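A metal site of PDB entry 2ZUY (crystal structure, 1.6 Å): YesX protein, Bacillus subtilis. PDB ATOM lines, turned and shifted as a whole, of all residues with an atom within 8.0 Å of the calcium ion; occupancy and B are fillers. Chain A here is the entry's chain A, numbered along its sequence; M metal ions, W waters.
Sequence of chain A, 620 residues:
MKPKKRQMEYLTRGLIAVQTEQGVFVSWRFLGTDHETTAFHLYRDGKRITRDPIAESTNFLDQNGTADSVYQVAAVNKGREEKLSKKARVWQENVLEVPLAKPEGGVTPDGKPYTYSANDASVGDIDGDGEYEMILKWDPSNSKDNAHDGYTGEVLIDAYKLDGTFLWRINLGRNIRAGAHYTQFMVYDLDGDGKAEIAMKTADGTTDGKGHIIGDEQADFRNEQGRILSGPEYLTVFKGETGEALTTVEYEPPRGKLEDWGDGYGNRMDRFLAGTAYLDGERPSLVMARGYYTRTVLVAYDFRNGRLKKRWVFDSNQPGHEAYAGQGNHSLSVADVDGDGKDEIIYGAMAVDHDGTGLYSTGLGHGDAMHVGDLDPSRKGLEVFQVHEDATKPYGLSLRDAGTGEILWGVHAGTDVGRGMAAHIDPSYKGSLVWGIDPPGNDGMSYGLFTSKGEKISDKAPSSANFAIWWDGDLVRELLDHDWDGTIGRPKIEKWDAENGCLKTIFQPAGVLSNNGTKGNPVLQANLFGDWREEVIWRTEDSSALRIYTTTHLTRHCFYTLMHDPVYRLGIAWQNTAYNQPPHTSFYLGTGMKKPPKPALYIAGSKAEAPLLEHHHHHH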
ATOM      1  N   HIS A 181      32.089 -33.954   4.613  1.00  0.00           N
ATOM      2  CA  HIS A 181      30.801 -34.523   4.211  1.00  0.00           C
ATOM      3  C   HIS A 181      30.240 -35.548   5.166  1.00  0.00           C
ATOM      4  O   HIS A 181      29.137 -36.066   4.934  1.00  0.00           O
ATOM      5  CB  HIS A 181      30.934 -35.111   2.801  1.00  0.00           C
ATOM      6  CG  HIS A 181      31.419 -34.107   1.814  1.00  0.00           C
ATOM      7  ND1 HIS A 181      30.670 -32.993   1.473  1.00  0.00           N
ATOM      8  CD2 HIS A 181      32.586 -33.988   1.159  1.00  0.00           C
ATOM      9  CE1 HIS A 181      31.345 -32.265   0.612  1.00  0.00           C
ATOM     10  NE2 HIS A 181      32.523 -32.839   0.411  1.00  0.00           N
ATOM     11  N   ARG A 271      27.357 -38.702   1.558  1.00  0.00           N
ATOM     12  CA  ARG A 271      27.224 -37.270   1.350  1.00  0.00           C
ATOM     13  C   ARG A 271      26.085 -36.787   2.228  1.00  0.00           C
ATOM     14  O   ARG A 271      24.911 -36.907   1.864  1.00  0.00           O
ATOM     15  CB  ARG A 271      26.961 -36.933  -0.115  1.00  0.00           C
ATOM     16  CG  ARG A 271      28.078 -37.341  -1.066  1.00  0.00           C
ATOM     17  CD  ARG A 271      29.367 -36.543  -0.896  1.00  0.00           C
ATOM     18  NE  ARG A 271      30.370 -37.079  -1.811  1.00  0.00           N
ATOM     19  CZ  ARG A 271      31.434 -36.415  -2.251  1.00  0.00           C
ATOM     20  NH1 ARG A 271      31.691 -35.169  -1.847  1.00  0.00           N
ATOM     21  NH2 ARG A 271      32.267 -37.022  -3.089  1.00  0.00           N
ATOM     22  N   TYR A 292      23.185 -36.597  -2.744  1.00  0.00           N
ATOM     23  CA  TYR A 292      22.742 -35.582  -3.705  1.00  0.00           C
ATOM     24  C   TYR A 292      23.110 -35.832  -5.164  1.00  0.00           C
ATOM     25  O   TYR A 292      22.377 -35.382  -6.041  1.00  0.00           O
ATOM     26  CB  TYR A 292      23.087 -34.141  -3.298  1.00  0.00           C
ATOM     27  CG  TYR A 292      24.401 -33.932  -2.585  1.00  0.00           C
ATOM     28  CD1 TYR A 292      24.426 -33.838  -1.191  1.00  0.00           C
ATOM     29  CD2 TYR A 292      25.586 -33.764  -3.280  1.00  0.00           C
ATOM     30  CE1 TYR A 292      25.616 -33.624  -0.508  1.00  0.00           C
ATOM     31  CE2 TYR A 292      26.790 -33.532  -2.602  1.00  0.00           C
ATOM     32  CZ  TYR A 292      26.788 -33.468  -1.219  1.00  0.00           C
ATOM     33  OH  TYR A 292      27.951 -33.243  -0.532  1.00  0.00           O
ATOM     34  N   TYR A 293      24.222 -36.517  -5.418  1.00  0.00           N
ATOM     35  CA  TYR A 293      24.649 -36.772  -6.806  1.00  0.00           C
ATOM     36  C   TYR A 293      23.710 -37.711  -7.542  1.00  0.00           C
ATOM     37  O   TYR A 293      23.466 -37.561  -8.738  1.00  0.00           O
ATOM     38  CB  TYR A 293      26.061 -37.354  -6.842  1.00  0.00           C
ATOM     39  CG  TYR A 293      27.104 -36.417  -6.301  1.00  0.00           C
ATOM     40  CD1 TYR A 293      27.483 -35.287  -7.018  1.00  0.00           C
ATOM     41  CD2 TYR A 293      27.714 -36.670  -5.065  1.00  0.00           C
ATOM     42  CE1 TYR A 293      28.454 -34.420  -6.524  1.00  0.00           C
ATOM     43  CE2 TYR A 293      28.669 -35.811  -4.563  1.00  0.00           C
ATOM     44  CZ  TYR A 293      29.043 -34.689  -5.300  1.00  0.00           C
ATOM     45  OH  TYR A 293      29.996 -33.853  -4.799  1.00  0.00           O
ATOM     46  N   GLY A 328      21.074 -31.737  -5.434  1.00  0.00           N
ATOM     47  CA  GLY A 328      21.531 -31.191  -4.166  1.00  0.00           C
ATOM     48  C   GLY A 328      22.919 -30.573  -4.232  1.00  0.00           C
ATOM     49  O   GLY A 328      23.753 -31.001  -5.037  1.00  0.00           O
ATOM     50  N   ASN A 329      23.144 -29.573  -3.393  1.00  0.00           N
ATOM     51  CA  ASN A 329      24.443 -28.904  -3.258  1.00  0.00           C
ATOM     52  C   ASN A 329      25.180 -29.492  -2.069  1.00  0.00           C
ATOM     53  O   ASN A 329      24.650 -30.364  -1.386  1.00  0.00           O
ATOM     54  CB  ASN A 329      24.243 -27.399  -3.007  1.00  0.00           C
ATOM     55  CG  ASN A 329      23.979 -26.613  -4.290  1.00  0.00           C
ATOM     56  OD1 ASN A 329      23.554 -27.164  -5.306  1.00  0.00           O
ATOM     57  ND2 ASN A 329      24.231 -25.301  -4.224  1.00  0.00           N
ATOM     58  N   HIS A 330      26.397 -28.999  -1.826  1.00  0.00           N
ATOM     59  CA  HIS A 330      27.117 -29.269  -0.577  1.00  0.00           C
ATOM     60  C   HIS A 330      26.620 -28.370   0.571  1.00  0.00           C
ATOM     61  O   HIS A 330      27.376 -28.033   1.483  1.00  0.00           O
ATOM     62  CB  HIS A 330      28.626 -29.042  -0.735  1.00  0.00           C
ATOM     63  CG  HIS A 330      29.260 -29.780  -1.884  1.00  0.00           C
ATOM     64  ND1 HIS A 330      29.529 -31.131  -1.848  1.00  0.00           N
ATOM     65  CD2 HIS A 330      29.743 -29.322  -3.057  1.00  0.00           C
ATOM     66  CE1 HIS A 330      30.121 -31.485  -2.976  1.00  0.00           C
ATOM     67  NE2 HIS A 330      30.274 -30.410  -3.721  1.00  0.00           N
ATOM     68  N   HIS A 366      23.483 -30.225  -9.141  1.00  0.00           N
ATOM     69  CA  HIS A 366      24.429 -29.932  -8.068  1.00  0.00           C
ATOM     70  C   HIS A 366      25.339 -28.724  -8.325  1.00  0.00           C
ATOM     71  O   HIS A 366      25.893 -28.565  -9.417  1.00  0.00           O
ATOM     72  CB  HIS A 366      25.308 -31.173  -7.864  1.00  0.00           C
ATOM     73  CG  HIS A 366      26.489 -30.932  -6.985  1.00  0.00           C
ATOM     74  ND1 HIS A 366      26.395 -30.901  -5.604  1.00  0.00           N
ATOM     75  CD2 HIS A 366      27.783 -30.687  -7.283  1.00  0.00           C
ATOM     76  CE1 HIS A 366      27.586 -30.656  -5.097  1.00  0.00           C
ATOM     77  NE2 HIS A 366      28.442 -30.507  -6.090  1.00  0.00           N
ATOM     78  N   GLY A 367      25.500 -27.918  -7.278  1.00  0.00           N
ATOM     79  CA  GLY A 367      26.496 -26.850  -7.229  1.00  0.00           C
ATOM     80  C   GLY A 367      27.146 -26.705  -5.855  1.00  0.00           C
ATOM     81  O   GLY A 367      26.779 -27.416  -4.908  1.00  0.00           O
ATOM     82  N   ASP A 368      28.094 -25.778  -5.746  1.00  0.00           N
ATOM     83  CA  ASP A 368      28.919 -25.628  -4.535  1.00  0.00           C
ATOM     84  C   ASP A 368      28.612 -24.417  -3.671  1.00  0.00           C
ATOM     85  O   ASP A 368      29.243 -24.208  -2.640  1.00  0.00           O
ATOM     86  CB  ASP A 368      30.412 -25.610  -4.897  1.00  0.00           C
ATOM     87  CG  ASP A 368      30.983 -26.987  -5.064  1.00  0.00           C
ATOM     88  OD1 ASP A 368      32.159 -27.208  -4.687  1.00  0.00           O
ATOM     89  OD2 ASP A 368      30.245 -27.851  -5.570  1.00  0.00           O
ATOM     90  N   ALA A 369      27.660 -23.596  -4.109  1.00  0.00           N
ATOM     91  CA  ALA A 369      27.236 -22.410  -3.369  1.00  0.00           C
ATOM     92  C   ALA A 369      25.788 -22.112  -3.710  1.00  0.00           C
ATOM     93  O   ALA A 369      25.348 -22.359  -4.835  1.00  0.00           O
ATOM     94  CB  ALA A 369      28.102 -21.210  -3.705  1.00  0.00           C
ATOM     95  N   HIS A 388      26.567 -23.823 -10.477  1.00  0.00           N
ATOM     96  CA  HIS A 388      26.390 -25.214 -10.884  1.00  0.00           C
ATOM     97  C   HIS A 388      27.726 -25.811 -11.340  1.00  0.00           C
ATOM     98  O   HIS A 388      28.556 -25.105 -11.910  1.00  0.00           O
ATOM     99  CB  HIS A 388      25.341 -25.320 -11.985  1.00  0.00           C
ATOM    100  CG  HIS A 388      24.018 -24.722 -11.602  1.00  0.00           C
ATOM    101  ND1 HIS A 388      23.091 -25.389 -10.838  1.00  0.00           N
ATOM    102  CD2 HIS A 388      23.485 -23.494 -11.851  1.00  0.00           C
ATOM    103  CE1 HIS A 388      22.032 -24.625 -10.650  1.00  0.00           C
ATOM    104  NE2 HIS A 388      22.257 -23.460 -11.246  1.00  0.00           N
ATOM    105  N   GLU A 389      27.896 -27.098 -11.086  1.00  0.00           N
ATOM    106  CA  GLU A 389      29.160 -27.795 -11.280  1.00  0.00           C
ATOM    107  C   GLU A 389      29.264 -28.545 -12.608  1.00  0.00           C
ATOM    108  O   GLU A 389      30.361 -28.720 -13.147  1.00  0.00           O
ATOM    109  CB  GLU A 389      29.341 -28.778 -10.124  1.00  0.00           C
ATOM    110  CG  GLU A 389      30.613 -29.610 -10.152  1.00  0.00           C
ATOM    111  CD  GLU A 389      30.821 -30.286  -8.824  1.00  0.00           C
ATOM    112  OE1 GLU A 389      30.800 -29.560  -7.816  1.00  0.00           O
ATOM    113  OE2 GLU A 389      30.974 -31.526  -8.792  1.00  0.00           O
ATOM    114  N   ASP A 390      28.128 -29.001 -13.110  1.00  0.00           N
ATOM    115  CA  ASP A 390      28.077 -29.879 -14.281  1.00  0.00           C
ATOM    116  C   ASP A 390      28.298 -29.055 -15.562  1.00  0.00           C
ATOM    117  O   ASP A 390      27.487 -28.206 -15.900  1.00  0.00           O
ATOM    118  CB  ASP A 390      26.732 -30.614 -14.298  1.00  0.00           C
ATOM    119  CG  ASP A 390      26.640 -31.707 -15.363  1.00  0.00           C
ATOM    120  OD1 ASP A 390      27.453 -31.727 -16.311  1.00  0.00           O
ATOM    121  OD2 ASP A 390      25.735 -32.544 -15.231  1.00  0.00           O
ATOM    122  N   ASP A 416      32.563 -26.054 -14.719  1.00  0.00           N
ATOM    123  CA  ASP A 416      32.261 -25.970 -13.291  1.00  0.00           C
ATOM    124  C   ASP A 416      32.448 -24.523 -12.830  1.00  0.00           C
ATOM    125  O   ASP A 416      33.527 -23.958 -12.972  1.00  0.00           O
ATOM    126  CB  ASP A 416      33.202 -26.915 -12.532  1.00  0.00           C
ATOM    127  CG  ASP A 416      33.036 -26.856 -11.015  1.00  0.00           C
ATOM    128  OD1 ASP A 416      32.108 -26.171 -10.516  1.00  0.00           O
ATOM    129  OD2 ASP A 416      33.852 -27.504 -10.323  1.00  0.00           O
ATOM    130  N   VAL A 417      31.385 -23.920 -12.293  1.00  0.00           N
ATOM    131  CA  VAL A 417      31.482 -22.621 -11.630  1.00  0.00           C
ATOM    132  C   VAL A 417      31.449 -22.880 -10.129  1.00  0.00           C
ATOM    133  O   VAL A 417      30.400 -23.153  -9.561  1.00  0.00           O
ATOM    134  CB  VAL A 417      30.357 -21.648 -12.054  1.00  0.00           C
ATOM    135  CG1 VAL A 417      30.474 -20.325 -11.322  1.00  0.00           C
ATOM    136  CG2 VAL A 417      30.409 -21.404 -13.555  1.00  0.00           C
ATOM    137  N   GLY A 418      32.629 -22.798  -9.503  1.00  0.00           N
ATOM    138  CA  GLY A 418      32.831 -23.316  -8.153  1.00  0.00           C
ATOM    139  C   GLY A 418      32.449 -22.422  -6.994  1.00  0.00           C
ATOM    140  O   GLY A 418      32.287 -22.914  -5.866  1.00  0.00           O
ATOM    141  N   LYS A 519      38.518 -23.494   0.991  1.00  0.00           N
ATOM    142  CA  LYS A 519      37.152 -23.017   1.310  1.00  0.00           C
ATOM    143  C   LYS A 519      37.175 -21.763   2.183  1.00  0.00           C
ATOM    144  O   LYS A 519      36.290 -20.901   2.093  1.00  0.00           O
ATOM    145  CB  LYS A 519      36.314 -24.128   1.960  1.00  0.00           C
ATOM    146  CG  LYS A 519      35.998 -25.325   1.031  1.00  0.00           C
ATOM    147  CD  LYS A 519      35.028 -24.943  -0.069  1.00  0.00           C
ATOM    148  CE  LYS A 519      34.811 -26.120  -1.022  1.00  0.00           C
ATOM    149  NZ  LYS A 519      33.958 -25.744  -2.190  1.00  0.00           N
ATOM    150  N   TYR A 579      29.961 -27.969   2.864  1.00  0.00           N
ATOM    151  CA  TYR A 579      30.759 -26.795   2.481  1.00  0.00           C
ATOM    152  C   TYR A 579      30.024 -25.536   2.931  1.00  0.00           C
ATOM    153  O   TYR A 579      29.124 -25.039   2.238  1.00  0.00           O
ATOM    154  CB  TYR A 579      31.035 -26.750   0.972  1.00  0.00           C
ATOM    155  CG  TYR A 579      31.917 -27.852   0.460  1.00  0.00           C
ATOM    156  CD1 TYR A 579      32.745 -28.590   1.319  1.00  0.00           C
ATOM    157  CD2 TYR A 579      31.935 -28.165  -0.912  1.00  0.00           C
ATOM    158  CE1 TYR A 579      33.560 -29.612   0.822  1.00  0.00           C
ATOM    159  CE2 TYR A 579      32.739 -29.182  -1.403  1.00  0.00           C
ATOM    160  CZ  TYR A 579      33.547 -29.910  -0.523  1.00  0.00           C
ATOM    161  OH  TYR A 579      34.343 -30.922  -0.999  1.00  0.00           O
HETATM  162 CA    CA M   1      30.551 -29.979  -5.797  1.00  0.00          CA
HETATM  163  O   HOH W   1      31.084 -32.095  -6.222  1.00  0.00           O
HETATM  164  O   HOH W   2      32.720 -29.605  -5.587  1.00  0.00           O
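Water W1 bridges OH of Tyr 293 (2.5 Å) and OE2 of Glu 389 (2.6 Å).
Within 4 Å of the calcium ion: His 330, His 366, Asp 368 and Glu 389.
The nearest printed residue that does not touch the calcium ion is Tyr 293 (4.04 Å).
The calcium ion is bound by OE1 of Glu 389 (2.1 Å).
NE2 of His 330 is bound to the calcium ion (2.1 Å).
OD2 of Asp 368 binds the calcium ion.
NE2 of His 366 is bound to the calcium ion.
Water W2 binds the calcium ion, 2.2 Å away.
Water W1 binds the calcium ion.
The calcium ion has six donor atoms within binding distance.
The backbone NH (N) of His 330 sits at hydrogen-bond distance from the backbone carbonyl oxygen (O) of Gly 367 (3.5 Å).
The backbone carbonyl oxygen (O) of His 330 lies within hydrogen-bond range of the backbone NH (N) of Tyr 579 (2.9 Å).
ND1 of His 330 lies within hydrogen-bond range of OH of Tyr 292, at 2.9 Å.
The side-chain carboxylate (OD1) of Asp 368 is in salt-bridge range of the side-chain amino group (NZ) of Lys 519, 3.4 Å away.
The backbone carbonyl oxygen of Gly 328 sits at hydrogen-bond distance from a ring nitrogen (ND1) of His 366.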
